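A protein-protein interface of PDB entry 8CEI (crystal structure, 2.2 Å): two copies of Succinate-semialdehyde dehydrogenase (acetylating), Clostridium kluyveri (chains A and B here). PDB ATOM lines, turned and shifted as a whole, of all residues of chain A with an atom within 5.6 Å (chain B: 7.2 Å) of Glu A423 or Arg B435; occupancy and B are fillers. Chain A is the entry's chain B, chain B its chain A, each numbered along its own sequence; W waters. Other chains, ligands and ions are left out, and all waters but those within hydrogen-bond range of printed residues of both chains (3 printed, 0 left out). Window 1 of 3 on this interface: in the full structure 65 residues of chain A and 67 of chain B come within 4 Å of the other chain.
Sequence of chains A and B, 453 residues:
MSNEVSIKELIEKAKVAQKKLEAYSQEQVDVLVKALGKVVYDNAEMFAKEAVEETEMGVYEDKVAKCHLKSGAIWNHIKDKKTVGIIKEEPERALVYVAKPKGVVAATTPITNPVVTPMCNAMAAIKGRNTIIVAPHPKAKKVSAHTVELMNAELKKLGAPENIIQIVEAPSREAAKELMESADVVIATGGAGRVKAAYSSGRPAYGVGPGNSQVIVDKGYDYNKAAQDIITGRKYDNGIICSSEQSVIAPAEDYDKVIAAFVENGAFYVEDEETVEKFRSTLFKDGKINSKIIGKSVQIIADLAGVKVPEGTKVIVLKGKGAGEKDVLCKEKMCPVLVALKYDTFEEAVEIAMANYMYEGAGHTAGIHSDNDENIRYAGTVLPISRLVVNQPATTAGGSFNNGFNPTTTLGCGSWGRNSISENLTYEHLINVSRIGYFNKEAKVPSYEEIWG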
ATOM      1  N   SER A 386      18.295 -22.452 -13.626  1.00  0.00           N
ATOM      2  CA  SER A 386      18.085 -21.022 -13.798  1.00  0.00           C
ATOM      3  C   SER A 386      17.053 -20.456 -12.835  1.00  0.00           C
ATOM      4  O   SER A 386      17.074 -19.249 -12.566  1.00  0.00           O
ATOM      5  CB  SER A 386      17.649 -20.716 -15.236  1.00  0.00           C
ATOM      6  OG  SER A 386      18.659 -21.074 -16.162  1.00  0.00           O
ATOM      7  N   ARG A 387      16.159 -21.293 -12.311  1.00  0.00           N
ATOM      8  CA  ARG A 387      15.092 -20.851 -11.427  1.00  0.00           C
ATOM      9  C   ARG A 387      14.897 -21.880 -10.325  1.00  0.00           C
ATOM     10  O   ARG A 387      14.741 -23.071 -10.610  1.00  0.00           O
ATOM     11  CB  ARG A 387      13.779 -20.658 -12.198  1.00  0.00           C
ATOM     12  CG  ARG A 387      13.806 -19.545 -13.237  1.00  0.00           C
ATOM     13  CD  ARG A 387      12.811 -19.816 -14.357  1.00  0.00           C
ATOM     14  NE  ARG A 387      13.239 -20.930 -15.196  1.00  0.00           N
ATOM     15  CZ  ARG A 387      13.965 -20.800 -16.298  1.00  0.00           C
ATOM     16  NH1 ARG A 387      14.339 -19.611 -16.741  1.00  0.00           N
ATOM     17  NH2 ARG A 387      14.329 -21.888 -16.969  1.00  0.00           N
ATOM     18  N   LEU A 388      14.916 -21.425  -9.076  1.00  0.00           N
ATOM     19  CA  LEU A 388      14.561 -22.249  -7.925  1.00  0.00           C
ATOM     20  C   LEU A 388      13.247 -21.712  -7.371  1.00  0.00           C
ATOM     21  O   LEU A 388      13.201 -20.601  -6.833  1.00  0.00           O
ATOM     22  CB  LEU A 388      15.657 -22.239  -6.861  1.00  0.00           C
ATOM     23  CG  LEU A 388      15.384 -23.119  -5.634  1.00  0.00           C
ATOM     24  CD1 LEU A 388      15.110 -24.559  -6.050  1.00  0.00           C
ATOM     25  CD2 LEU A 388      16.535 -23.063  -4.640  1.00  0.00           C
ATOM     26  N   VAL A 389      12.186 -22.498  -7.517  1.00  0.00           N
ATOM     27  CA  VAL A 389      10.844 -22.092  -7.119  1.00  0.00           C
ATOM     28  C   VAL A 389      10.592 -22.600  -5.705  1.00  0.00           C
ATOM     29  O   VAL A 389      10.656 -23.808  -5.451  1.00  0.00           O
ATOM     30  CB  VAL A 389       9.796 -22.629  -8.104  1.00  0.00           C
ATOM     31  CG1 VAL A 389       8.419 -22.142  -7.739  1.00  0.00           C
ATOM     32  CG2 VAL A 389      10.146 -22.205  -9.520  1.00  0.00           C
ATOM     33  N   PHE A 405       9.543 -13.773 -10.593  1.00  0.00           N
ATOM     34  CA  PHE A 405       9.923 -14.193 -11.935  1.00  0.00           C
ATOM     35  C   PHE A 405       9.193 -13.354 -12.977  1.00  0.00           C
ATOM     36  O   PHE A 405       8.008 -13.044 -12.829  1.00  0.00           O
ATOM     37  CB  PHE A 405       9.614 -15.676 -12.146  1.00  0.00           C
ATOM     38  CG  PHE A 405      10.357 -16.592 -11.215  1.00  0.00           C
ATOM     39  CD1 PHE A 405      11.730 -16.752 -11.327  1.00  0.00           C
ATOM     40  CD2 PHE A 405       9.682 -17.305 -10.237  1.00  0.00           C
ATOM     41  CE1 PHE A 405      12.417 -17.596 -10.474  1.00  0.00           C
ATOM     42  CE2 PHE A 405      10.361 -18.154  -9.381  1.00  0.00           C
ATOM     43  CZ  PHE A 405      11.731 -18.300  -9.500  1.00  0.00           C
ATOM     44  N   ASN A 406       9.909 -12.980 -14.030  1.00  0.00           N
ATOM     45  CA  ASN A 406       9.304 -12.179 -15.086  1.00  0.00           C
ATOM     46  C   ASN A 406       8.314 -13.027 -15.875  1.00  0.00           C
ATOM     47  O   ASN A 406       8.641 -14.158 -16.258  1.00  0.00           O
ATOM     48  CB  ASN A 406      10.377 -11.611 -16.013  1.00  0.00           C
ATOM     49  CG  ASN A 406      11.283 -10.614 -15.313  1.00  0.00           C
ATOM     50  OD1 ASN A 406      10.895  -9.996 -14.322  1.00  0.00           O
ATOM     51  ND2 ASN A 406      12.495 -10.452 -15.829  1.00  0.00           N
ATOM     52  N   THR A 410       8.654 -18.213 -22.711  1.00  0.00           N
ATOM     53  CA  THR A 410       9.943 -18.707 -23.195  1.00  0.00           C
ATOM     54  C   THR A 410      10.932 -18.632 -22.035  1.00  0.00           C
ATOM     55  O   THR A 410      11.433 -17.552 -21.705  1.00  0.00           O
ATOM     56  CB  THR A 410      10.424 -17.888 -24.392  1.00  0.00           C
ATOM     57  OG1 THR A 410       9.454 -17.957 -25.446  1.00  0.00           O
ATOM     58  CG2 THR A 410      11.761 -18.406 -24.900  1.00  0.00           C
ATOM     59  N   LEU A 411      11.215 -19.778 -21.418  1.00  0.00           N
ATOM     60  CA  LEU A 411      12.064 -19.849 -20.230  1.00  0.00           C
ATOM     61  C   LEU A 411      13.454 -20.315 -20.654  1.00  0.00           C
ATOM     62  O   LEU A 411      13.670 -21.501 -20.912  1.00  0.00           O
ATOM     63  CB  LEU A 411      11.458 -20.780 -19.183  1.00  0.00           C
ATOM     64  CG  LEU A 411      10.189 -20.331 -18.449  1.00  0.00           C
ATOM     65  CD1 LEU A 411       8.940 -20.509 -19.305  1.00  0.00           C
ATOM     66  CD2 LEU A 411      10.043 -21.074 -17.127  1.00  0.00           C
ATOM     67  N   GLY A 412      14.397 -19.377 -20.717  1.00  0.00           N
ATOM     68  CA  GLY A 412      15.757 -19.724 -21.082  1.00  0.00           C
ATOM     69  C   GLY A 412      16.442 -20.550 -20.010  1.00  0.00           C
ATOM     70  O   GLY A 412      16.155 -20.433 -18.818  1.00  0.00           O
ATOM     71  N   CYS A 413      17.378 -21.398 -20.448  1.00  0.00           N
ATOM     72  CA  CYS A 413      18.030 -22.359 -19.565  1.00  0.00           C
ATOM     73  C   CYS A 413      19.545 -22.178 -19.509  1.00  0.00           C
ATOM     74  O   CYS A 413      20.260 -23.108 -19.124  1.00  0.00           O
ATOM     75  CB  CYS A 413      17.684 -23.788 -19.989  1.00  0.00           C
ATOM     76  SG  CYS A 413      15.919 -24.169 -19.913  1.00  0.00           S
ATOM     77  N   GLY A 414      20.048 -21.005 -19.889  1.00  0.00           N
ATOM     78  CA  GLY A 414      21.464 -20.726 -19.746  1.00  0.00           C
ATOM     79  C   GLY A 414      22.354 -21.608 -20.612  1.00  0.00           C
ATOM     80  O   GLY A 414      21.921 -22.242 -21.579  1.00  0.00           O
ATOM     81  N   ILE A 421      20.709 -16.960 -22.410  1.00  0.00           N
ATOM     82  CA  ILE A 421      20.376 -16.402 -21.107  1.00  0.00           C
ATOM     83  C   ILE A 421      19.869 -17.511 -20.196  1.00  0.00           C
ATOM     84  O   ILE A 421      19.292 -18.504 -20.651  1.00  0.00           O
ATOM     85  CB  ILE A 421      19.325 -15.272 -21.206  1.00  0.00           C
ATOM     86  CG1 ILE A 421      18.044 -15.790 -21.868  1.00  0.00           C
ATOM     87  CG2 ILE A 421      19.891 -14.076 -21.957  1.00  0.00           C
ATOM     88  CD1 ILE A 421      16.901 -14.798 -21.858  1.00  0.00           C
ATOM     89  N   SER A 422      20.091 -17.329 -18.896  1.00  0.00           N
ATOM     90  CA  SER A 422      19.558 -18.237 -17.889  1.00  0.00           C
ATOM     91  C   SER A 422      18.397 -17.571 -17.162  1.00  0.00           C
ATOM     92  O   SER A 422      18.337 -17.579 -15.928  1.00  0.00           O
ATOM     93  CB  SER A 422      20.651 -18.647 -16.900  1.00  0.00           C
ATOM     94  OG  SER A 422      21.203 -17.513 -16.254  1.00  0.00           O
ATOM     95  N   GLU A 423      17.475 -16.984 -17.923  1.00  0.00           N
ATOM     96  CA  GLU A 423      16.348 -16.276 -17.342  1.00  0.00           C
ATOM     97  C   GLU A 423      15.176 -16.317 -18.310  1.00  0.00           C
ATOM     98  O   GLU A 423      15.299 -16.750 -19.459  1.00  0.00           O
ATOM     99  CB  GLU A 423      16.712 -14.828 -16.999  1.00  0.00           C
ATOM    100  CG  GLU A 423      17.254 -14.027 -18.172  1.00  0.00           C
ATOM    101  CD  GLU A 423      17.427 -12.555 -17.846  1.00  0.00           C
ATOM    102  OE1 GLU A 423      16.740 -12.064 -16.925  1.00  0.00           O
ATOM    103  OE2 GLU A 423      18.248 -11.889 -18.509  1.00  0.00           O
ATOM    104  N   ASN A 424      14.030 -15.849 -17.822  1.00  0.00           N
ATOM    105  CA  ASN A 424      12.824 -15.784 -18.632  1.00  0.00           C
ATOM    106  C   ASN A 424      12.956 -14.718 -19.715  1.00  0.00           C
ATOM    107  O   ASN A 424      13.522 -13.644 -19.489  1.00  0.00           O
ATOM    108  CB  ASN A 424      11.622 -15.487 -17.737  1.00  0.00           C
ATOM    109  CG  ASN A 424      11.299 -16.632 -16.793  1.00  0.00           C
ATOM    110  OD1 ASN A 424      11.980 -17.661 -16.789  1.00  0.00           O
ATOM    111  ND2 ASN A 424      10.261 -16.456 -15.981  1.00  0.00           N
ATOM    112  N   LEU A 425      12.424 -15.019 -20.900  1.00  0.00           N
ATOM    113  CA  LEU A 425      12.520 -14.112 -22.038  1.00  0.00           C
ATOM    114  C   LEU A 425      11.530 -12.963 -21.887  1.00  0.00           C
ATOM    115  O   LEU A 425      10.342 -13.186 -21.626  1.00  0.00           O
ATOM    116  CB  LEU A 425      12.254 -14.862 -23.342  1.00  0.00           C
ATOM    117  CG  LEU A 425      12.342 -14.027 -24.623  1.00  0.00           C
ATOM    118  CD1 LEU A 425      13.792 -13.789 -25.009  1.00  0.00           C
ATOM    119  CD2 LEU A 425      11.576 -14.687 -25.761  1.00  0.00           C
ATOM    120  N   HIS A 429      15.273  -8.511 -23.919  1.00  0.00           N
ATOM    121  CA  HIS A 429      16.181  -9.298 -24.740  1.00  0.00           C
ATOM    122  C   HIS A 429      15.991  -9.054 -26.231  1.00  0.00           C
ATOM    123  O   HIS A 429      16.764  -9.588 -27.034  1.00  0.00           O
ATOM    124  CB  HIS A 429      16.009 -10.785 -24.429  1.00  0.00           C
ATOM    125  CG  HIS A 429      16.077 -11.104 -22.967  1.00  0.00           C
ATOM    126  ND1 HIS A 429      14.952 -11.298 -22.195  1.00  0.00           N
ATOM    127  CD2 HIS A 429      17.135 -11.245 -22.135  1.00  0.00           C
ATOM    128  CE1 HIS A 429      15.314 -11.553 -20.950  1.00  0.00           C
ATOM    129  NE2 HIS A 429      16.633 -11.527 -20.887  1.00  0.00           N
ATOM    130  N   GLU B  90      17.102  -9.079  -3.413  1.00  0.00           N
ATOM    131  CA  GLU B  90      16.041  -8.175  -3.861  1.00  0.00           C
ATOM    132  C   GLU B  90      14.746  -8.570  -3.170  1.00  0.00           C
ATOM    133  O   GLU B  90      13.899  -9.267  -3.742  1.00  0.00           O
ATOM    134  CB  GLU B  90      15.896  -8.203  -5.385  1.00  0.00           C
ATOM    135  CG  GLU B  90      15.007  -7.098  -5.942  1.00  0.00           C
ATOM    136  CD  GLU B  90      15.073  -6.998  -7.454  1.00  0.00           C
ATOM    137  OE1 GLU B  90      15.687  -7.883  -8.084  1.00  0.00           O
ATOM    138  OE2 GLU B  90      14.516  -6.029  -8.014  1.00  0.00           O
ATOM    139  N   ARG B  93      11.047  -7.946  -4.639  1.00  0.00           N
ATOM    140  CA  ARG B  93      10.524  -8.954  -5.551  1.00  0.00           C
ATOM    141  C   ARG B  93      10.654 -10.364  -4.992  1.00  0.00           C
ATOM    142  O   ARG B  93      10.346 -11.328  -5.701  1.00  0.00           O
ATOM    143  CB  ARG B  93      11.228  -8.868  -6.906  1.00  0.00           C
ATOM    144  CG  ARG B  93      11.171  -7.496  -7.557  1.00  0.00           C
ATOM    145  CD  ARG B  93      11.566  -7.571  -9.022  1.00  0.00           C
ATOM    146  NE  ARG B  93      10.570  -8.274  -9.820  1.00  0.00           N
ATOM    147  CZ  ARG B  93      10.701  -8.550 -11.110  1.00  0.00           C
ATOM    148  NH1 ARG B  93      11.793  -8.215 -11.781  1.00  0.00           N
ATOM    149  NH2 ARG B  93       9.715  -9.176 -11.745  1.00  0.00           N
ATOM    150  N   ALA B  94      11.100 -10.505  -3.740  1.00  0.00           N
ATOM    151  CA  ALA B  94      11.336 -11.812  -3.124  1.00  0.00           C
ATOM    152  C   ALA B  94      12.268 -12.663  -3.983  1.00  0.00           C
ATOM    153  O   ALA B  94      12.034 -13.853  -4.204  1.00  0.00           O
ATOM    154  CB  ALA B  94      10.019 -12.542  -2.854  1.00  0.00           C
ATOM    155  N   LEU B  95      13.337 -12.043  -4.476  1.00  0.00           N
ATOM    156  CA  LEU B  95      14.283 -12.700  -5.364  1.00  0.00           C
ATOM    157  C   LEU B  95      15.671 -12.728  -4.743  1.00  0.00           C
ATOM    158  O   LEU B  95      16.075 -11.804  -4.032  1.00  0.00           O
ATOM    159  CB  LEU B  95      14.350 -11.998  -6.728  1.00  0.00           C
ATOM    160  CG  LEU B  95      13.159 -12.161  -7.672  1.00  0.00           C
ATOM    161  CD1 LEU B  95      13.399 -11.377  -8.953  1.00  0.00           C
ATOM    162  CD2 LEU B  95      12.910 -13.630  -7.979  1.00  0.00           C
ATOM    163  N   VAL B  96      16.395 -13.809  -5.024  1.00  0.00           N
ATOM    164  CA  VAL B  96      17.796 -13.959  -4.651  1.00  0.00           C
ATOM    165  C   VAL B  96      18.559 -14.400  -5.891  1.00  0.00           C
ATOM    166  O   VAL B  96      18.179 -15.382  -6.541  1.00  0.00           O
ATOM    167  CB  VAL B  96      17.982 -14.972  -3.505  1.00  0.00           C
ATOM    168  CG1 VAL B  96      19.456 -15.268  -3.294  1.00  0.00           C
ATOM    169  CG2 VAL B  96      17.356 -14.443  -2.223  1.00  0.00           C
ATOM    170  N   TYR B  97      19.622 -13.674  -6.223  1.00  0.00           N
ATOM    171  CA  TYR B  97      20.387 -13.904  -7.440  1.00  0.00           C
ATOM    172  C   TYR B  97      21.627 -14.736  -7.143  1.00  0.00           C
ATOM    173  O   TYR B  97      22.337 -14.488  -6.164  1.00  0.00           O
ATOM    174  CB  TYR B  97      20.792 -12.577  -8.086  1.00  0.00           C
ATOM    175  CG  TYR B  97      19.624 -11.754  -8.580  1.00  0.00           C
ATOM    176  CD1 TYR B  97      18.906 -10.940  -7.713  1.00  0.00           C
ATOM    177  CD2 TYR B  97      19.240 -11.787  -9.915  1.00  0.00           C
ATOM    178  CE1 TYR B  97      17.838 -10.184  -8.159  1.00  0.00           C
ATOM    179  CE2 TYR B  97      18.174 -11.034 -10.371  1.00  0.00           C
ATOM    180  CZ  TYR B  97      17.477 -10.234  -9.489  1.00  0.00           C
ATOM    181  OH  TYR B  97      16.414  -9.482  -9.937  1.00  0.00           O
ATOM    182  N   VAL B  98      21.886 -15.721  -8.001  1.00  0.00           N
ATOM    183  CA  VAL B  98      22.995 -16.653  -7.839  1.00  0.00           C
ATOM    184  C   VAL B  98      23.827 -16.636  -9.113  1.00  0.00           C
ATOM    185  O   VAL B  98      23.290 -16.811 -10.213  1.00  0.00           O
ATOM    186  CB  VAL B  98      22.503 -18.083  -7.541  1.00  0.00           C
ATOM    187  CG1 VAL B  98      23.683 -19.026  -7.373  1.00  0.00           C
ATOM    188  CG2 VAL B  98      21.618 -18.098  -6.302  1.00  0.00           C
ATOM    189  N   LYS B 100      26.561 -18.339 -11.486  1.00  0.00           N
ATOM    190  CA  LYS B 100      27.096 -19.652 -11.797  1.00  0.00           C
ATOM    191  C   LYS B 100      27.913 -19.596 -13.080  1.00  0.00           C
ATOM    192  O   LYS B 100      27.565 -18.857 -14.009  1.00  0.00           O
ATOM    193  CB  LYS B 100      25.972 -20.686 -11.943  1.00  0.00           C
ATOM    194  CG  LYS B 100      25.216 -20.960 -10.657  1.00  0.00           C
ATOM    195  CD  LYS B 100      24.538 -22.316 -10.709  1.00  0.00           C
ATOM    196  CE  LYS B 100      23.953 -22.686  -9.361  1.00  0.00           C
ATOM    197  NZ  LYS B 100      22.767 -21.853  -9.027  1.00  0.00           N
ATOM    198  N   ASN B 432      26.047 -17.398 -15.829  1.00  0.00           N
ATOM    199  CA  ASN B 432      24.601 -17.541 -15.766  1.00  0.00           C
ATOM    200  C   ASN B 432      24.121 -17.050 -14.407  1.00  0.00           C
ATOM    201  O   ASN B 432      24.604 -17.512 -13.369  1.00  0.00           O
ATOM    202  CB  ASN B 432      24.182 -18.997 -15.981  1.00  0.00           C
ATOM    203  CG  ASN B 432      24.490 -19.494 -17.378  1.00  0.00           C
ATOM    204  OD1 ASN B 432      25.180 -20.499 -17.552  1.00  0.00           O
ATOM    205  ND2 ASN B 432      23.976 -18.796 -18.385  1.00  0.00           N
ATOM    206  N   VAL B 433      23.185 -16.109 -14.416  1.00  0.00           N
ATOM    207  CA  VAL B 433      22.605 -15.570 -13.193  1.00  0.00           C
ATOM    208  C   VAL B 433      21.275 -16.275 -12.967  1.00  0.00           C
ATOM    209  O   VAL B 433      20.323 -16.089 -13.733  1.00  0.00           O
ATOM    210  CB  VAL B 433      22.428 -14.047 -13.269  1.00  0.00           C
ATOM    211  CG1 VAL B 433      21.717 -13.533 -12.027  1.00  0.00           C
ATOM    212  CG2 VAL B 433      23.782 -13.368 -13.430  1.00  0.00           C
ATOM    213  N   SER B 434      21.213 -17.095 -11.923  1.00  0.00           N
ATOM    214  CA  SER B 434      19.993 -17.791 -11.554  1.00  0.00           C
ATOM    215  C   SER B 434      19.232 -16.990 -10.502  1.00  0.00           C
ATOM    216  O   SER B 434      19.760 -16.065  -9.884  1.00  0.00           O
ATOM    217  CB  SER B 434      20.314 -19.193 -11.039  1.00  0.00           C
ATOM    218  OG  SER B 434      21.027 -19.935 -12.013  1.00  0.00           O
ATOM    219  N   ARG B 435      17.969 -17.359 -10.303  1.00  0.00           N
ATOM    220  CA  ARG B 435      17.086 -16.642  -9.395  1.00  0.00           C
ATOM    221  C   ARG B 435      16.389 -17.623  -8.467  1.00  0.00           C
ATOM    222  O   ARG B 435      15.792 -18.602  -8.925  1.00  0.00           O
ATOM    223  CB  ARG B 435      16.044 -15.825 -10.166  1.00  0.00           C
ATOM    224  CG  ARG B 435      16.606 -14.606 -10.870  1.00  0.00           C
ATOM    225  CD  ARG B 435      15.599 -14.025 -11.846  1.00  0.00           C
ATOM    226  NE  ARG B 435      16.087 -12.794 -12.455  1.00  0.00           N
ATOM    227  CZ  ARG B 435      16.960 -12.748 -13.451  1.00  0.00           C
ATOM    228  NH1 ARG B 435      17.472 -13.850 -13.972  1.00  0.00           N
ATOM    229  NH2 ARG B 435      17.333 -11.565 -13.932  1.00  0.00           N
ATOM    230  N   ILE B 436      16.472 -17.358  -7.169  1.00  0.00           N
ATOM    231  CA  ILE B 436      15.663 -18.057  -6.177  1.00  0.00           C
ATOM    232  C   ILE B 436      14.404 -17.232  -5.955  1.00  0.00           C
ATOM    233  O   ILE B 436      14.476 -16.078  -5.518  1.00  0.00           O
ATOM    234  CB  ILE B 436      16.435 -18.258  -4.865  1.00  0.00           C
ATOM    235  CG1 ILE B 436      17.737 -19.019  -5.121  1.00  0.00           C
ATOM    236  CG2 ILE B 436      15.569 -18.991  -3.848  1.00  0.00           C
ATOM    237  CD1 ILE B 436      18.610 -19.166  -3.892  1.00  0.00           C
ATOM    238  N   GLY B 437      13.251 -17.814  -6.275  1.00  0.00           N
ATOM    239  CA  GLY B 437      11.995 -17.101  -6.164  1.00  0.00           C
ATOM    240  C   GLY B 437      11.151 -17.546  -4.990  1.00  0.00           C
ATOM    241  O   GLY B 437      10.523 -18.608  -5.033  1.00  0.00           O
ATOM    242  N   TYR B 438      11.131 -16.743  -3.931  1.00  0.00           N
ATOM    243  CA  TYR B 438      10.319 -17.049  -2.768  1.00  0.00           C
ATOM    244  C   TYR B 438       8.860 -16.686  -3.027  1.00  0.00           C
ATOM    245  O   TYR B 438       8.525 -15.968  -3.973  1.00  0.00           O
ATOM    246  CB  TYR B 438      10.842 -16.309  -1.538  1.00  0.00           C
ATOM    247  CG  TYR B 438      12.220 -16.746  -1.104  1.00  0.00           C
ATOM    248  CD1 TYR B 438      13.356 -16.142  -1.622  1.00  0.00           C
ATOM    249  CD2 TYR B 438      12.386 -17.765  -0.175  1.00  0.00           C
ATOM    250  CE1 TYR B 438      14.619 -16.540  -1.228  1.00  0.00           C
ATOM    251  CE2 TYR B 438      13.644 -18.169   0.226  1.00  0.00           C
ATOM    252  CZ  TYR B 438      14.758 -17.552  -0.304  1.00  0.00           C
ATOM    253  OH  TYR B 438      16.015 -17.951   0.091  1.00  0.00           O
HETATM  254  O   HOH W   1      12.949 -11.756 -12.384  1.00  0.00           O
HETATM  255  O   HOH W   2      14.335  -8.331 -14.038  1.00  0.00           O
HETATM  256  O   HOH W   3      16.903 -16.881 -14.014  1.00  0.00           O
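No position is printed for both chains.
Of the 13 pairs that touch across the chains among the printed residues, none has its exchanged pair printed and touching as well.
Along chain A the printed residues that touch a printed residue of chain B span positions 386 to 423.
Among the printed residues, 13 pairs touch across the chains.
Among the printed residues, Asp or Glu carboxylates within 4 Å of a Lys or Arg side-chain nitrogen of the other chain: Glu A423 with Arg B435 (3.1 Å).
Water W3 lies within hydrogen-bond range of the backbone carbonyl oxygen (O) of Ser A422, the backbone carbonyl oxygen (O) of Ser A386 and the guanidinium group (NH1) of Arg B435.
Water W1 lies within hydrogen-bond range of the guanidinium group (NE) of Arg B435 (3.3 Å) and the side-chain amide oxygen (OD1) of Asn A406 (3.3 Å).
Water W2 lies within hydrogen-bond range of ND2 of Asn A406 and NH1 of Arg B93.
The side-chain amide oxygen of Asn A406 lies within hydrogen-bond range of the guanidinium group of Arg B93 (3.0 Å).
The side-chain carboxylate (OE1) of Glu A423 is in salt-bridge range of the guanidinium group (NH2) of Arg B435 (3.1 Å).
The backbone carbonyl oxygen of Val B433 sits at hydrogen-bond distance from the side-chain hydroxyl of Ser A422 (3.0 Å).
The backbone carbonyl oxygen (O) of Arg B435 sits at hydrogen-bond distance from the backbone NH (N) of Leu A388, at 3.0 Å.
O of Leu A388 is in hydrogen-bond range of N of Gly B437, at 2.8 Å.
The backbone NH (N) of Arg B435 is in hydrogen-bond range of the backbone carbonyl oxygen (O) of Ser A386 (3.1 Å).
Of the printed residues of chain B, Arg A387 touches Arg B435 (3.4 Å).
Of the printed residues of chain B, Phe A405 touches Arg B435 (3.8 Å) and Gly B437 (3.6 Å).
Of chain B, only Arg B435 (3.1 Å) comes within 4 Å of Glu A423.
Of the printed residues of chain A, Arg B93 touches Asn A406 (3.0 Å).
Printed residues of chain A within 4 Å of Ser B434: Ser A386 (3.4 Å).
Arg B435 touches just these residues of chain A: Ser A386, Arg A387, Leu A388, Phe A405 and Glu A423.
Printed residues of chain A within 4 Å of Gly B437: Leu A388 and Phe A405.
Tyr B438 touches none of the printed residues of chain A.
The nearest residue of chain B that does not touch Glu A423 is Val B433 (5.0 Å).
The nearest residue of chain A that does not touch Arg B435 is Ser A422 (4.3 Å).
Ser A386 touches Ser B434 (O to CA, 3.4 Å).
Arg A387 touches Arg B435 (CA to O, 3.4 Å).
Leu A388 touches Ile B436 (O to CA, 3.6 Å).
CE1 of Phe A405 touches O of Arg B435 (3.8 Å).
CZ of Phe A405 touches CA of Gly B437 (3.6 Å).
Asn B432 touches Gly A414.
Ser A422 touches Asn B432 (OG to CB, 3.3 Å).
O of Lys B100 is in hydrogen-bond range of N of Asn B432 (2.8 Å).
N of Ser B434 sits at hydrogen-bond distance from O of Val B98.
The backbone NH (N) of Ile B436 is in hydrogen-bond range of the backbone carbonyl oxygen (O) of Val B96 (2.7 Å).
NH1 of Arg A387 sits at hydrogen-bond distance from O of Gly A412.
OE2 of Glu A423 lies within hydrogen-bond range of NE2 of His A429.
N of Gly A412 lies within hydrogen-bond range of O of Glu A423, at 3.0 Å.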
